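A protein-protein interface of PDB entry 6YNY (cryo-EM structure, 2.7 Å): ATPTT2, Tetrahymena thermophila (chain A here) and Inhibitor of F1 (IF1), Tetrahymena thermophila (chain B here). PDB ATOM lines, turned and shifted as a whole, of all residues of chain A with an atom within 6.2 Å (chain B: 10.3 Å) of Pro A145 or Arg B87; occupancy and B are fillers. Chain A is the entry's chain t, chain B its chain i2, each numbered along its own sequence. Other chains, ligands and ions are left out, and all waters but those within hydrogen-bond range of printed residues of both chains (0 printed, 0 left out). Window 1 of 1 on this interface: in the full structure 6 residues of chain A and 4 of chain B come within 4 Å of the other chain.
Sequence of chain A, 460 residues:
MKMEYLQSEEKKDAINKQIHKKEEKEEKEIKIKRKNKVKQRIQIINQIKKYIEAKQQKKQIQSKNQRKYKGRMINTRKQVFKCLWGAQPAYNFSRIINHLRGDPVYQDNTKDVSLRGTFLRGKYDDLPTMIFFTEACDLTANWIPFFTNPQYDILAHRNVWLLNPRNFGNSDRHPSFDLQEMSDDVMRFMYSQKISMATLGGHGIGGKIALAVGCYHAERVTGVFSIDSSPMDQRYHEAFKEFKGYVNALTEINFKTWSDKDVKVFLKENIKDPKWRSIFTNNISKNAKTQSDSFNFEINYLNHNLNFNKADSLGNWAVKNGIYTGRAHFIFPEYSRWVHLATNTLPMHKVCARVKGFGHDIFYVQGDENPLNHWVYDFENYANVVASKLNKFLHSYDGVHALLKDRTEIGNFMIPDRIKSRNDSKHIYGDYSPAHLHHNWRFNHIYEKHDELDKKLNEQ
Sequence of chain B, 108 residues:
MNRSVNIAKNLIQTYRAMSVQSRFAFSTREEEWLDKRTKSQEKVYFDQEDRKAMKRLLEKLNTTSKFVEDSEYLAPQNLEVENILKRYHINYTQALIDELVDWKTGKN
O of Ala A141 sits at hydrogen-bond distance from NE of Arg B87, 3.5 Å away. The side-chain carboxylate (OD1) of Asp A378 is in hydrogen-bond range of a ring nitrogen (NE2) of His B89, 2.7 Å away.
O of Arg B87 lies within hydrogen-bond range of NE2 of His B89, 3.1 Å away.
Asn A142 touches Arg B87 (OD1 to CD, 3.2 Å). Arg B87 touches Pro A145. Tyr B88 touches Pro A145 (CD1 to CB, 3.7 Å). His B89 touches Tyr A377 (CE1 to O, 3.1 Å).
No residue of chain B comes within 4 Å of Ile A144. Of chain B, only Arg B87 (3.7 Å) and Tyr B88 (3.7 Å) come within 4 Å of Pro A145. Of the printed residues of chain B, Tyr A377 touches His B89. Of the printed residues of chain B, Asp A378 touches His B89 (2.7 Å). Of the printed residues of chain A, Arg B87 touches Ala A141 (3.5 Å), Asn A142 (3.2 Å) and Pro A145 (3.7 Å). Printed residues of chain A within 4 Å of Tyr B88: Pro A145. The nearest residue of chain A that does not touch Arg B87 is Ile A144 (4.9 Å). The nearest printed residue of chain A that does not touch Tyr B88 is Ile A144 (4.04 Å).
Hydrophobic or aromatic side chains of chain A that line the printed part of chain B: Ala A141 and Pro A145. Hydrophobic or aromatic side chains of chain B that line the printed part of chain A: Tyr B88 and His B89. Among the printed residues, 6 pairs touch across the chains. Among the printed residues, no Asp or Glu carboxylate lies within 4 Å of a Lys or Arg side-chain nitrogen of the other chain.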
ATOM      1  N   LEU A 139      -7.370 -20.478  -0.156  1.00  0.00           N
ATOM      2  CA  LEU A 139      -7.748 -20.503  -1.559  1.00  0.00           C
ATOM      3  C   LEU A 139      -6.814 -19.655  -2.407  1.00  0.00           C
ATOM      4  O   LEU A 139      -6.380 -18.574  -2.000  1.00  0.00           O
ATOM      5  CB  LEU A 139      -9.178 -20.002  -1.723  1.00  0.00           C
ATOM      6  CG  LEU A 139     -10.240 -20.799  -0.976  1.00  0.00           C
ATOM      7  CD1 LEU A 139     -11.567 -20.107  -1.120  1.00  0.00           C
ATOM      8  CD2 LEU A 139     -10.312 -22.218  -1.499  1.00  0.00           C
ATOM      9  N   THR A 140      -6.515 -20.160  -3.601  1.00  0.00           N
ATOM     10  CA  THR A 140      -5.722 -19.402  -4.558  1.00  0.00           C
ATOM     11  C   THR A 140      -6.502 -18.219  -5.115  1.00  0.00           C
ATOM     12  O   THR A 140      -5.911 -17.178  -5.420  1.00  0.00           O
ATOM     13  CB  THR A 140      -5.264 -20.332  -5.684  1.00  0.00           C
ATOM     14  OG1 THR A 140      -3.982 -20.885  -5.364  1.00  0.00           O
ATOM     15  CG2 THR A 140      -5.194 -19.613  -7.010  1.00  0.00           C
ATOM     16  N   ALA A 141      -7.821 -18.359  -5.249  1.00  0.00           N
ATOM     17  CA  ALA A 141      -8.625 -17.287  -5.821  1.00  0.00           C
ATOM     18  C   ALA A 141      -8.505 -15.999  -5.023  1.00  0.00           C
ATOM     19  O   ALA A 141      -8.598 -14.906  -5.593  1.00  0.00           O
ATOM     20  CB  ALA A 141     -10.083 -17.724  -5.896  1.00  0.00           C
ATOM     21  N   ASN A 142      -8.301 -16.100  -3.708  1.00  0.00           N
ATOM     22  CA  ASN A 142      -8.249 -14.904  -2.878  1.00  0.00           C
ATOM     23  C   ASN A 142      -7.103 -13.983  -3.277  1.00  0.00           C
ATOM     24  O   ASN A 142      -7.172 -12.773  -3.040  1.00  0.00           O
ATOM     25  CB  ASN A 142      -8.127 -15.295  -1.409  1.00  0.00           C
ATOM     26  CG  ASN A 142      -9.390 -15.918  -0.868  1.00  0.00           C
ATOM     27  OD1 ASN A 142     -10.491 -15.609  -1.319  1.00  0.00           O
ATOM     28  ND2 ASN A 142      -9.242 -16.799   0.108  1.00  0.00           N
ATOM     29  N   TRP A 143      -6.046 -14.530  -3.872  1.00  0.00           N
ATOM     30  CA  TRP A 143      -4.904 -13.733  -4.295  1.00  0.00           C
ATOM     31  C   TRP A 143      -5.041 -13.177  -5.704  1.00  0.00           C
ATOM     32  O   TRP A 143      -4.190 -12.387  -6.123  1.00  0.00           O
ATOM     33  CB  TRP A 143      -3.622 -14.562  -4.210  1.00  0.00           C
ATOM     34  CG  TRP A 143      -3.088 -14.695  -2.829  1.00  0.00           C
ATOM     35  CD1 TRP A 143      -3.278 -15.736  -1.974  1.00  0.00           C
ATOM     36  CD2 TRP A 143      -2.272 -13.749  -2.134  1.00  0.00           C
ATOM     37  NE1 TRP A 143      -2.631 -15.498  -0.789  1.00  0.00           N
ATOM     38  CE2 TRP A 143      -2.005 -14.284  -0.862  1.00  0.00           C
ATOM     39  CE3 TRP A 143      -1.743 -12.501  -2.462  1.00  0.00           C
ATOM     40  CZ2 TRP A 143      -1.233 -13.617   0.078  1.00  0.00           C
ATOM     41  CZ3 TRP A 143      -0.977 -11.842  -1.527  1.00  0.00           C
ATOM     42  CH2 TRP A 143      -0.730 -12.400  -0.273  1.00  0.00           C
ATOM     43  N   ILE A 144      -6.082 -13.559  -6.443  1.00  0.00           N
ATOM     44  CA  ILE A 144      -6.246 -13.056  -7.805  1.00  0.00           C
ATOM     45  C   ILE A 144      -6.413 -11.543  -7.832  1.00  0.00           C
ATOM     46  O   ILE A 144      -5.726 -10.882  -8.628  1.00  0.00           O
ATOM     47  CB  ILE A 144      -7.405 -13.788  -8.503  1.00  0.00           C
ATOM     48  CG1 ILE A 144      -7.072 -15.270  -8.646  1.00  0.00           C
ATOM     49  CG2 ILE A 144      -7.661 -13.177  -9.855  1.00  0.00           C
ATOM     50  CD1 ILE A 144      -8.167 -16.089  -9.261  1.00  0.00           C
ATOM     51  N   PRO A 145      -7.291 -10.935  -7.033  1.00  0.00           N
ATOM     52  CA  PRO A 145      -7.417  -9.473  -7.092  1.00  0.00           C
ATOM     53  C   PRO A 145      -6.132  -8.750  -6.739  1.00  0.00           C
ATOM     54  O   PRO A 145      -5.928  -7.614  -7.185  1.00  0.00           O
ATOM     55  CB  PRO A 145      -8.538  -9.179  -6.087  1.00  0.00           C
ATOM     56  CG  PRO A 145      -8.617 -10.369  -5.230  1.00  0.00           C
ATOM     57  CD  PRO A 145      -8.249 -11.522  -6.085  1.00  0.00           C
ATOM     58  N   PHE A 146      -5.257  -9.374  -5.951  1.00  0.00           N
ATOM     59  CA  PHE A 146      -3.977  -8.756  -5.638  1.00  0.00           C
ATOM     60  C   PHE A 146      -3.074  -8.727  -6.863  1.00  0.00           C
ATOM     61  O   PHE A 146      -2.463  -7.698  -7.172  1.00  0.00           O
ATOM     62  CB  PHE A 146      -3.304  -9.501  -4.487  1.00  0.00           C
ATOM     63  CG  PHE A 146      -1.969  -8.944  -4.107  1.00  0.00           C
ATOM     64  CD1 PHE A 146      -1.879  -7.844  -3.283  1.00  0.00           C
ATOM     65  CD2 PHE A 146      -0.804  -9.520  -4.571  1.00  0.00           C
ATOM     66  CE1 PHE A 146      -0.660  -7.329  -2.934  1.00  0.00           C
ATOM     67  CE2 PHE A 146       0.419  -9.007  -4.222  1.00  0.00           C
ATOM     68  CZ  PHE A 146       0.492  -7.912  -3.403  1.00  0.00           C
ATOM     69  N   PHE A 147      -2.982  -9.847  -7.578  1.00  0.00           N
ATOM     70  CA  PHE A 147      -2.128  -9.927  -8.752  1.00  0.00           C
ATOM     71  C   PHE A 147      -2.780  -9.375 -10.013  1.00  0.00           C
ATOM     72  O   PHE A 147      -2.109  -9.298 -11.045  1.00  0.00           O
ATOM     73  CB  PHE A 147      -1.707 -11.373  -8.999  1.00  0.00           C
ATOM     74  CG  PHE A 147      -0.694 -11.888  -8.025  1.00  0.00           C
ATOM     75  CD1 PHE A 147      -1.075 -12.684  -6.965  1.00  0.00           C
ATOM     76  CD2 PHE A 147       0.643 -11.583  -8.174  1.00  0.00           C
ATOM     77  CE1 PHE A 147      -0.146 -13.160  -6.076  1.00  0.00           C
ATOM     78  CE2 PHE A 147       1.576 -12.058  -7.284  1.00  0.00           C
ATOM     79  CZ  PHE A 147       1.182 -12.847  -6.236  1.00  0.00           C
ATOM     80  N   THR A 148      -4.054  -8.993  -9.963  1.00  0.00           N
ATOM     81  CA  THR A 148      -4.761  -8.442 -11.111  1.00  0.00           C
ATOM     82  C   THR A 148      -5.316  -7.063 -10.795  1.00  0.00           C
ATOM     83  O   THR A 148      -6.429  -6.715 -11.191  1.00  0.00           O
ATOM     84  CB  THR A 148      -5.892  -9.365 -11.558  1.00  0.00           C
ATOM     85  OG1 THR A 148      -6.736  -9.666 -10.441  1.00  0.00           O
ATOM     86  CG2 THR A 148      -5.351 -10.645 -12.148  1.00  0.00           C
ATOM     87  N   ASN A 149      -4.539  -6.253 -10.083  1.00  0.00           N
ATOM     88  CA  ASN A 149      -4.952  -4.908  -9.728  1.00  0.00           C
ATOM     89  C   ASN A 149      -4.168  -3.910 -10.564  1.00  0.00           C
ATOM     90  O   ASN A 149      -2.929  -3.938 -10.536  1.00  0.00           O
ATOM     91  CB  ASN A 149      -4.735  -4.648  -8.244  1.00  0.00           C
ATOM     92  CG  ASN A 149      -5.326  -3.335  -7.793  1.00  0.00           C
ATOM     93  OD1 ASN A 149      -5.901  -2.592  -8.584  1.00  0.00           O
ATOM     94  ND2 ASN A 149      -5.205  -3.048  -6.509  1.00  0.00           N
ATOM     95  N   TYR A 152      -1.408  -1.838  -8.686  1.00  0.00           N
ATOM     96  CA  TYR A 152      -0.138  -2.506  -8.440  1.00  0.00           C
ATOM     97  C   TYR A 152       0.580  -2.819  -9.746  1.00  0.00           C
ATOM     98  O   TYR A 152       1.776  -2.544  -9.888  1.00  0.00           O
ATOM     99  CB  TYR A 152      -0.374  -3.783  -7.636  1.00  0.00           C
ATOM    100  CG  TYR A 152      -1.169  -3.572  -6.370  1.00  0.00           C
ATOM    101  CD1 TYR A 152      -1.915  -4.599  -5.821  1.00  0.00           C
ATOM    102  CD2 TYR A 152      -1.173  -2.348  -5.723  1.00  0.00           C
ATOM    103  CE1 TYR A 152      -2.641  -4.414  -4.671  1.00  0.00           C
ATOM    104  CE2 TYR A 152      -1.898  -2.156  -4.573  1.00  0.00           C
ATOM    105  CZ  TYR A 152      -2.630  -3.192  -4.051  1.00  0.00           C
ATOM    106  OH  TYR A 152      -3.355  -3.004  -2.901  1.00  0.00           O
ATOM    107  N   TYR A 377      -3.594  -9.258   1.854  1.00  0.00           N
ATOM    108  CA  TYR A 377      -4.320  -8.936   0.632  1.00  0.00           C
ATOM    109  C   TYR A 377      -5.692  -8.338   0.913  1.00  0.00           C
ATOM    110  O   TYR A 377      -6.270  -7.700   0.027  1.00  0.00           O
ATOM    111  CB  TYR A 377      -4.450 -10.180  -0.248  1.00  0.00           C
ATOM    112  CG  TYR A 377      -5.164 -11.346   0.386  1.00  0.00           C
ATOM    113  CD1 TYR A 377      -6.544 -11.391   0.444  1.00  0.00           C
ATOM    114  CD2 TYR A 377      -4.456 -12.420   0.897  1.00  0.00           C
ATOM    115  CE1 TYR A 377      -7.196 -12.455   1.011  1.00  0.00           C
ATOM    116  CE2 TYR A 377      -5.101 -13.489   1.462  1.00  0.00           C
ATOM    117  CZ  TYR A 377      -6.471 -13.505   1.516  1.00  0.00           C
ATOM    118  OH  TYR A 377      -7.118 -14.574   2.083  1.00  0.00           O
ATOM    119  N   ASP A 378      -6.229  -8.529   2.118  1.00  0.00           N
ATOM    120  CA  ASP A 378      -7.543  -7.988   2.443  1.00  0.00           C
ATOM    121  C   ASP A 378      -7.486  -6.495   2.737  1.00  0.00           C
ATOM    122  O   ASP A 378      -8.383  -5.747   2.333  1.00  0.00           O
ATOM    123  CB  ASP A 378      -8.140  -8.729   3.637  1.00  0.00           C
ATOM    124  CG  ASP A 378      -8.599 -10.129   3.288  1.00  0.00           C
ATOM    125  OD1 ASP A 378      -8.994 -10.356   2.126  1.00  0.00           O
ATOM    126  OD2 ASP A 378      -8.575 -11.001   4.180  1.00  0.00           O
ATOM    127  N   LEU B  79     -25.322 -18.580  -3.475  1.00  0.00           N
ATOM    128  CA  LEU B  79     -24.496 -17.587  -2.735  1.00  0.00           C
ATOM    129  C   LEU B  79     -23.097 -17.510  -3.357  1.00  0.00           C
ATOM    130  O   LEU B  79     -22.149 -17.145  -2.634  1.00  0.00           O
ATOM    131  CB  LEU B  79     -24.431 -17.990  -1.257  1.00  0.00           C
ATOM    132  CG  LEU B  79     -23.631 -19.254  -0.935  1.00  0.00           C
ATOM    133  CD1 LEU B  79     -23.685 -20.256  -2.078  1.00  0.00           C
ATOM    134  CD2 LEU B  79     -22.189 -18.914  -0.591  1.00  0.00           C
ATOM    135  N   GLU B  80     -22.980 -17.825  -4.653  1.00  0.00           N
ATOM    136  CA  GLU B  80     -21.703 -17.809  -5.414  1.00  0.00           C
ATOM    137  C   GLU B  80     -21.273 -16.357  -5.655  1.00  0.00           C
ATOM    138  O   GLU B  80     -20.088 -16.047  -5.422  1.00  0.00           O
ATOM    139  CB  GLU B  80     -21.864 -18.558  -6.739  1.00  0.00           C
ATOM    140  CG  GLU B  80     -21.388 -19.999  -6.682  1.00  0.00           C
ATOM    141  CD  GLU B  80     -21.874 -20.871  -7.826  1.00  0.00           C
ATOM    142  OE1 GLU B  80     -21.985 -20.353  -8.955  1.00  0.00           O
ATOM    143  OE2 GLU B  80     -22.141 -22.064  -7.586  1.00  0.00           O
ATOM    144  N   VAL B  81     -22.204 -15.510  -6.104  1.00  0.00           N
ATOM    145  CA  VAL B  81     -21.956 -14.101  -6.388  1.00  0.00           C
ATOM    146  C   VAL B  81     -21.527 -13.368  -5.129  1.00  0.00           C
ATOM    147  O   VAL B  81     -20.781 -12.384  -5.196  1.00  0.00           O
ATOM    148  CB  VAL B  81     -23.207 -13.454  -7.007  1.00  0.00           C
ATOM    149  CG1 VAL B  81     -22.974 -11.976  -7.251  1.00  0.00           C
ATOM    150  CG2 VAL B  81     -23.573 -14.156  -8.290  1.00  0.00           C
ATOM    151  N   GLU B  82     -22.027 -13.833  -3.981  1.00  0.00           N
ATOM    152  CA  GLU B  82     -21.731 -13.257  -2.641  1.00  0.00           C
ATOM    153  C   GLU B  82     -20.245 -13.423  -2.299  1.00  0.00           C
ATOM    154  O   GLU B  82     -19.656 -12.454  -1.778  1.00  0.00           O
ATOM    155  CB  GLU B  82     -22.602 -13.927  -1.576  1.00  0.00           C
ATOM    156  CG  GLU B  82     -23.150 -12.955  -0.547  1.00  0.00           C
ATOM    157  CD  GLU B  82     -24.569 -13.251  -0.092  1.00  0.00           C
ATOM    158  OE1 GLU B  82     -24.995 -14.417  -0.210  1.00  0.00           O
ATOM    159  OE2 GLU B  82     -25.245 -12.315   0.380  1.00  0.00           O
ATOM    160  N   ASN B  83     -19.662 -14.595  -2.578  1.00  0.00           N
ATOM    161  CA  ASN B  83     -18.268 -14.890  -2.260  1.00  0.00           C
ATOM    162  C   ASN B  83     -17.321 -14.192  -3.226  1.00  0.00           C
ATOM    163  O   ASN B  83     -16.322 -13.594  -2.809  1.00  0.00           O
ATOM    164  CB  ASN B  83     -18.036 -16.400  -2.278  1.00  0.00           C
ATOM    165  CG  ASN B  83     -18.846 -17.127  -1.227  1.00  0.00           C
ATOM    166  OD1 ASN B  83     -19.219 -16.549  -0.206  1.00  0.00           O
ATOM    167  ND2 ASN B  83     -19.120 -18.402  -1.470  1.00  0.00           N
ATOM    168  N   ILE B  84     -17.614 -14.263  -4.525  1.00  0.00           N
ATOM    169  CA  ILE B  84     -16.716 -13.689  -5.524  1.00  0.00           C
ATOM    170  C   ILE B  84     -16.548 -12.192  -5.297  1.00  0.00           C
ATOM    171  O   ILE B  84     -15.438 -11.655  -5.394  1.00  0.00           O
ATOM    172  CB  ILE B  84     -17.232 -13.995  -6.943  1.00  0.00           C
ATOM    173  CG1 ILE B  84     -16.260 -13.462  -7.989  1.00  0.00           C
ATOM    174  CG2 ILE B  84     -18.591 -13.373  -7.157  1.00  0.00           C
ATOM    175  CD1 ILE B  84     -16.553 -13.950  -9.384  1.00  0.00           C
ATOM    176  N   LEU B  85     -17.643 -11.492  -4.998  1.00  0.00           N
ATOM    177  CA  LEU B  85     -17.549 -10.054  -4.768  1.00  0.00           C
ATOM    178  C   LEU B  85     -16.787  -9.752  -3.486  1.00  0.00           C
ATOM    179  O   LEU B  85     -16.032  -8.775  -3.420  1.00  0.00           O
ATOM    180  CB  LEU B  85     -18.944  -9.435  -4.718  1.00  0.00           C
ATOM    181  CG  LEU B  85     -19.722  -9.428  -6.033  1.00  0.00           C
ATOM    182  CD1 LEU B  85     -21.136  -8.938  -5.810  1.00  0.00           C
ATOM    183  CD2 LEU B  85     -19.024  -8.564  -7.065  1.00  0.00           C
ATOM    184  N   LYS B  86     -16.972 -10.578  -2.453  1.00  0.00           N
ATOM    185  CA  LYS B  86     -16.252 -10.363  -1.204  1.00  0.00           C
ATOM    186  C   LYS B  86     -14.748 -10.485  -1.404  1.00  0.00           C
ATOM    187  O   LYS B  86     -13.975  -9.814  -0.713  1.00  0.00           O
ATOM    188  CB  LYS B  86     -16.738 -11.354  -0.148  1.00  0.00           C
ATOM    189  CG  LYS B  86     -18.104 -11.011   0.424  1.00  0.00           C
ATOM    190  CD  LYS B  86     -18.535 -11.981   1.515  1.00  0.00           C
ATOM    191  CE  LYS B  86     -18.707 -13.388   0.977  1.00  0.00           C
ATOM    192  NZ  LYS B  86     -19.302 -14.305   1.987  1.00  0.00           N
ATOM    193  N   ARG B  87     -14.316 -11.334  -2.338  1.00  0.00           N
ATOM    194  CA  ARG B  87     -12.890 -11.465  -2.611  1.00  0.00           C
ATOM    195  C   ARG B  87     -12.292 -10.139  -3.055  1.00  0.00           C
ATOM    196  O   ARG B  87     -11.168  -9.795  -2.673  1.00  0.00           O
ATOM    197  CB  ARG B  87     -12.644 -12.534  -3.671  1.00  0.00           C
ATOM    198  CG  ARG B  87     -13.070 -13.918  -3.263  1.00  0.00           C
ATOM    199  CD  ARG B  87     -12.181 -14.946  -3.912  1.00  0.00           C
ATOM    200  NE  ARG B  87     -12.043 -14.717  -5.346  1.00  0.00           N
ATOM    201  CZ  ARG B  87     -12.821 -15.262  -6.274  1.00  0.00           C
ATOM    202  NH1 ARG B  87     -12.609 -14.986  -7.551  1.00  0.00           N
ATOM    203  NH2 ARG B  87     -13.806 -16.082  -5.933  1.00  0.00           N
ATOM    204  N   TYR B  88     -13.024  -9.387  -3.869  1.00  0.00           N
ATOM    205  CA  TYR B  88     -12.577  -8.082  -4.326  1.00  0.00           C
ATOM    206  C   TYR B  88     -12.895  -6.975  -3.334  1.00  0.00           C
ATOM    207  O   TYR B  88     -12.742  -5.797  -3.674  1.00  0.00           O
ATOM    208  CB  TYR B  88     -13.197  -7.771  -5.689  1.00  0.00           C
ATOM    209  CG  TYR B  88     -12.627  -8.617  -6.798  1.00  0.00           C
ATOM    210  CD1 TYR B  88     -11.719  -8.089  -7.701  1.00  0.00           C
ATOM    211  CD2 TYR B  88     -12.981  -9.951  -6.931  1.00  0.00           C
ATOM    212  CE1 TYR B  88     -11.188  -8.861  -8.709  1.00  0.00           C
ATOM    213  CE2 TYR B  88     -12.453 -10.731  -7.935  1.00  0.00           C
ATOM    214  CZ  TYR B  88     -11.557 -10.181  -8.821  1.00  0.00           C
ATOM    215  OH  TYR B  88     -11.033 -10.960  -9.823  1.00  0.00           O
ATOM    216  N   HIS B  89     -13.376  -7.339  -2.144  1.00  0.00           N
ATOM    217  CA  HIS B  89     -13.616  -6.396  -1.021  1.00  0.00           C
ATOM    218  C   HIS B  89     -14.447  -5.211  -1.516  1.00  0.00           C
ATOM    219  O   HIS B  89     -14.171  -4.074  -1.083  1.00  0.00           O
ATOM    220  CB  HIS B  89     -12.283  -5.949  -0.405  1.00  0.00           C
ATOM    221  CG  HIS B  89     -11.302  -7.058  -0.225  1.00  0.00           C
ATOM    222  ND1 HIS B  89      -9.960  -6.913  -0.520  1.00  0.00           N
ATOM    223  CD2 HIS B  89     -11.459  -8.326   0.215  1.00  0.00           C
ATOM    224  CE1 HIS B  89      -9.333  -8.044  -0.268  1.00  0.00           C
ATOM    225  NE2 HIS B  89     -10.230  -8.927   0.183  1.00  0.00           N
ATOM    226  N   ILE B  90     -15.421  -5.472  -2.388  1.00  0.00           N
ATOM    227  CA  ILE B  90     -16.323  -4.466  -2.935  1.00  0.00           C
ATOM    228  C   ILE B  90     -17.645  -4.565  -2.191  1.00  0.00           C
ATOM    229  O   ILE B  90     -18.222  -5.653  -2.079  1.00  0.00           O
ATOM    230  CB  ILE B  90     -16.537  -4.663  -4.445  1.00  0.00           C
ATOM    231  CG1 ILE B  90     -15.198  -4.782  -5.168  1.00  0.00           C
ATOM    232  CG2 ILE B  90     -17.331  -3.510  -5.023  1.00  0.00           C
ATOM    233  CD1 ILE B  90     -15.328  -4.879  -6.670  1.00  0.00           C
ATOM    234  N   ASN B  91     -18.125  -3.433  -1.682  1.00  0.00           N
ATOM    235  CA  ASN B  91     -19.409  -3.407  -0.996  1.00  0.00           C
ATOM    236  C   ASN B  91     -20.526  -3.652  -2.003  1.00  0.00           C
ATOM    237  O   ASN B  91     -20.639  -2.933  -3.002  1.00  0.00           O
ATOM    238  CB  ASN B  91     -19.607  -2.071  -0.287  1.00  0.00           C
ATOM    239  CG  ASN B  91     -18.541  -1.801   0.754  1.00  0.00           C
ATOM    240  OD1 ASN B  91     -18.663  -2.218   1.906  1.00  0.00           O
ATOM    241  ND2 ASN B  91     -17.488  -1.097   0.355  1.00  0.00           N
ATOM    242  N   TYR B  92     -21.350  -4.661  -1.740  1.00  0.00           N
ATOM    243  CA  TYR B  92     -22.409  -5.070  -2.650  1.00  0.00           C
ATOM    244  C   TYR B  92     -23.759  -4.903  -1.970  1.00  0.00           C
ATOM    245  O   TYR B  92     -23.930  -5.301  -0.813  1.00  0.00           O
ATOM    246  CB  TYR B  92     -22.219  -6.522  -3.090  1.00  0.00           C
ATOM    247  CG  TYR B  92     -22.067  -7.495  -1.943  1.00  0.00           C
ATOM    248  CD1 TYR B  92     -23.177  -8.080  -1.354  1.00  0.00           C
ATOM    249  CD2 TYR B  92     -20.814  -7.829  -1.454  1.00  0.00           C
ATOM    250  CE1 TYR B  92     -23.044  -8.969  -0.308  1.00  0.00           C
ATOM    251  CE2 TYR B  92     -20.671  -8.717  -0.408  1.00  0.00           C
ATOM    252  CZ  TYR B  92     -21.789  -9.284   0.162  1.00  0.00           C
ATOM    253  OH  TYR B  92     -21.649 -10.170   1.204  1.00  0.00           O
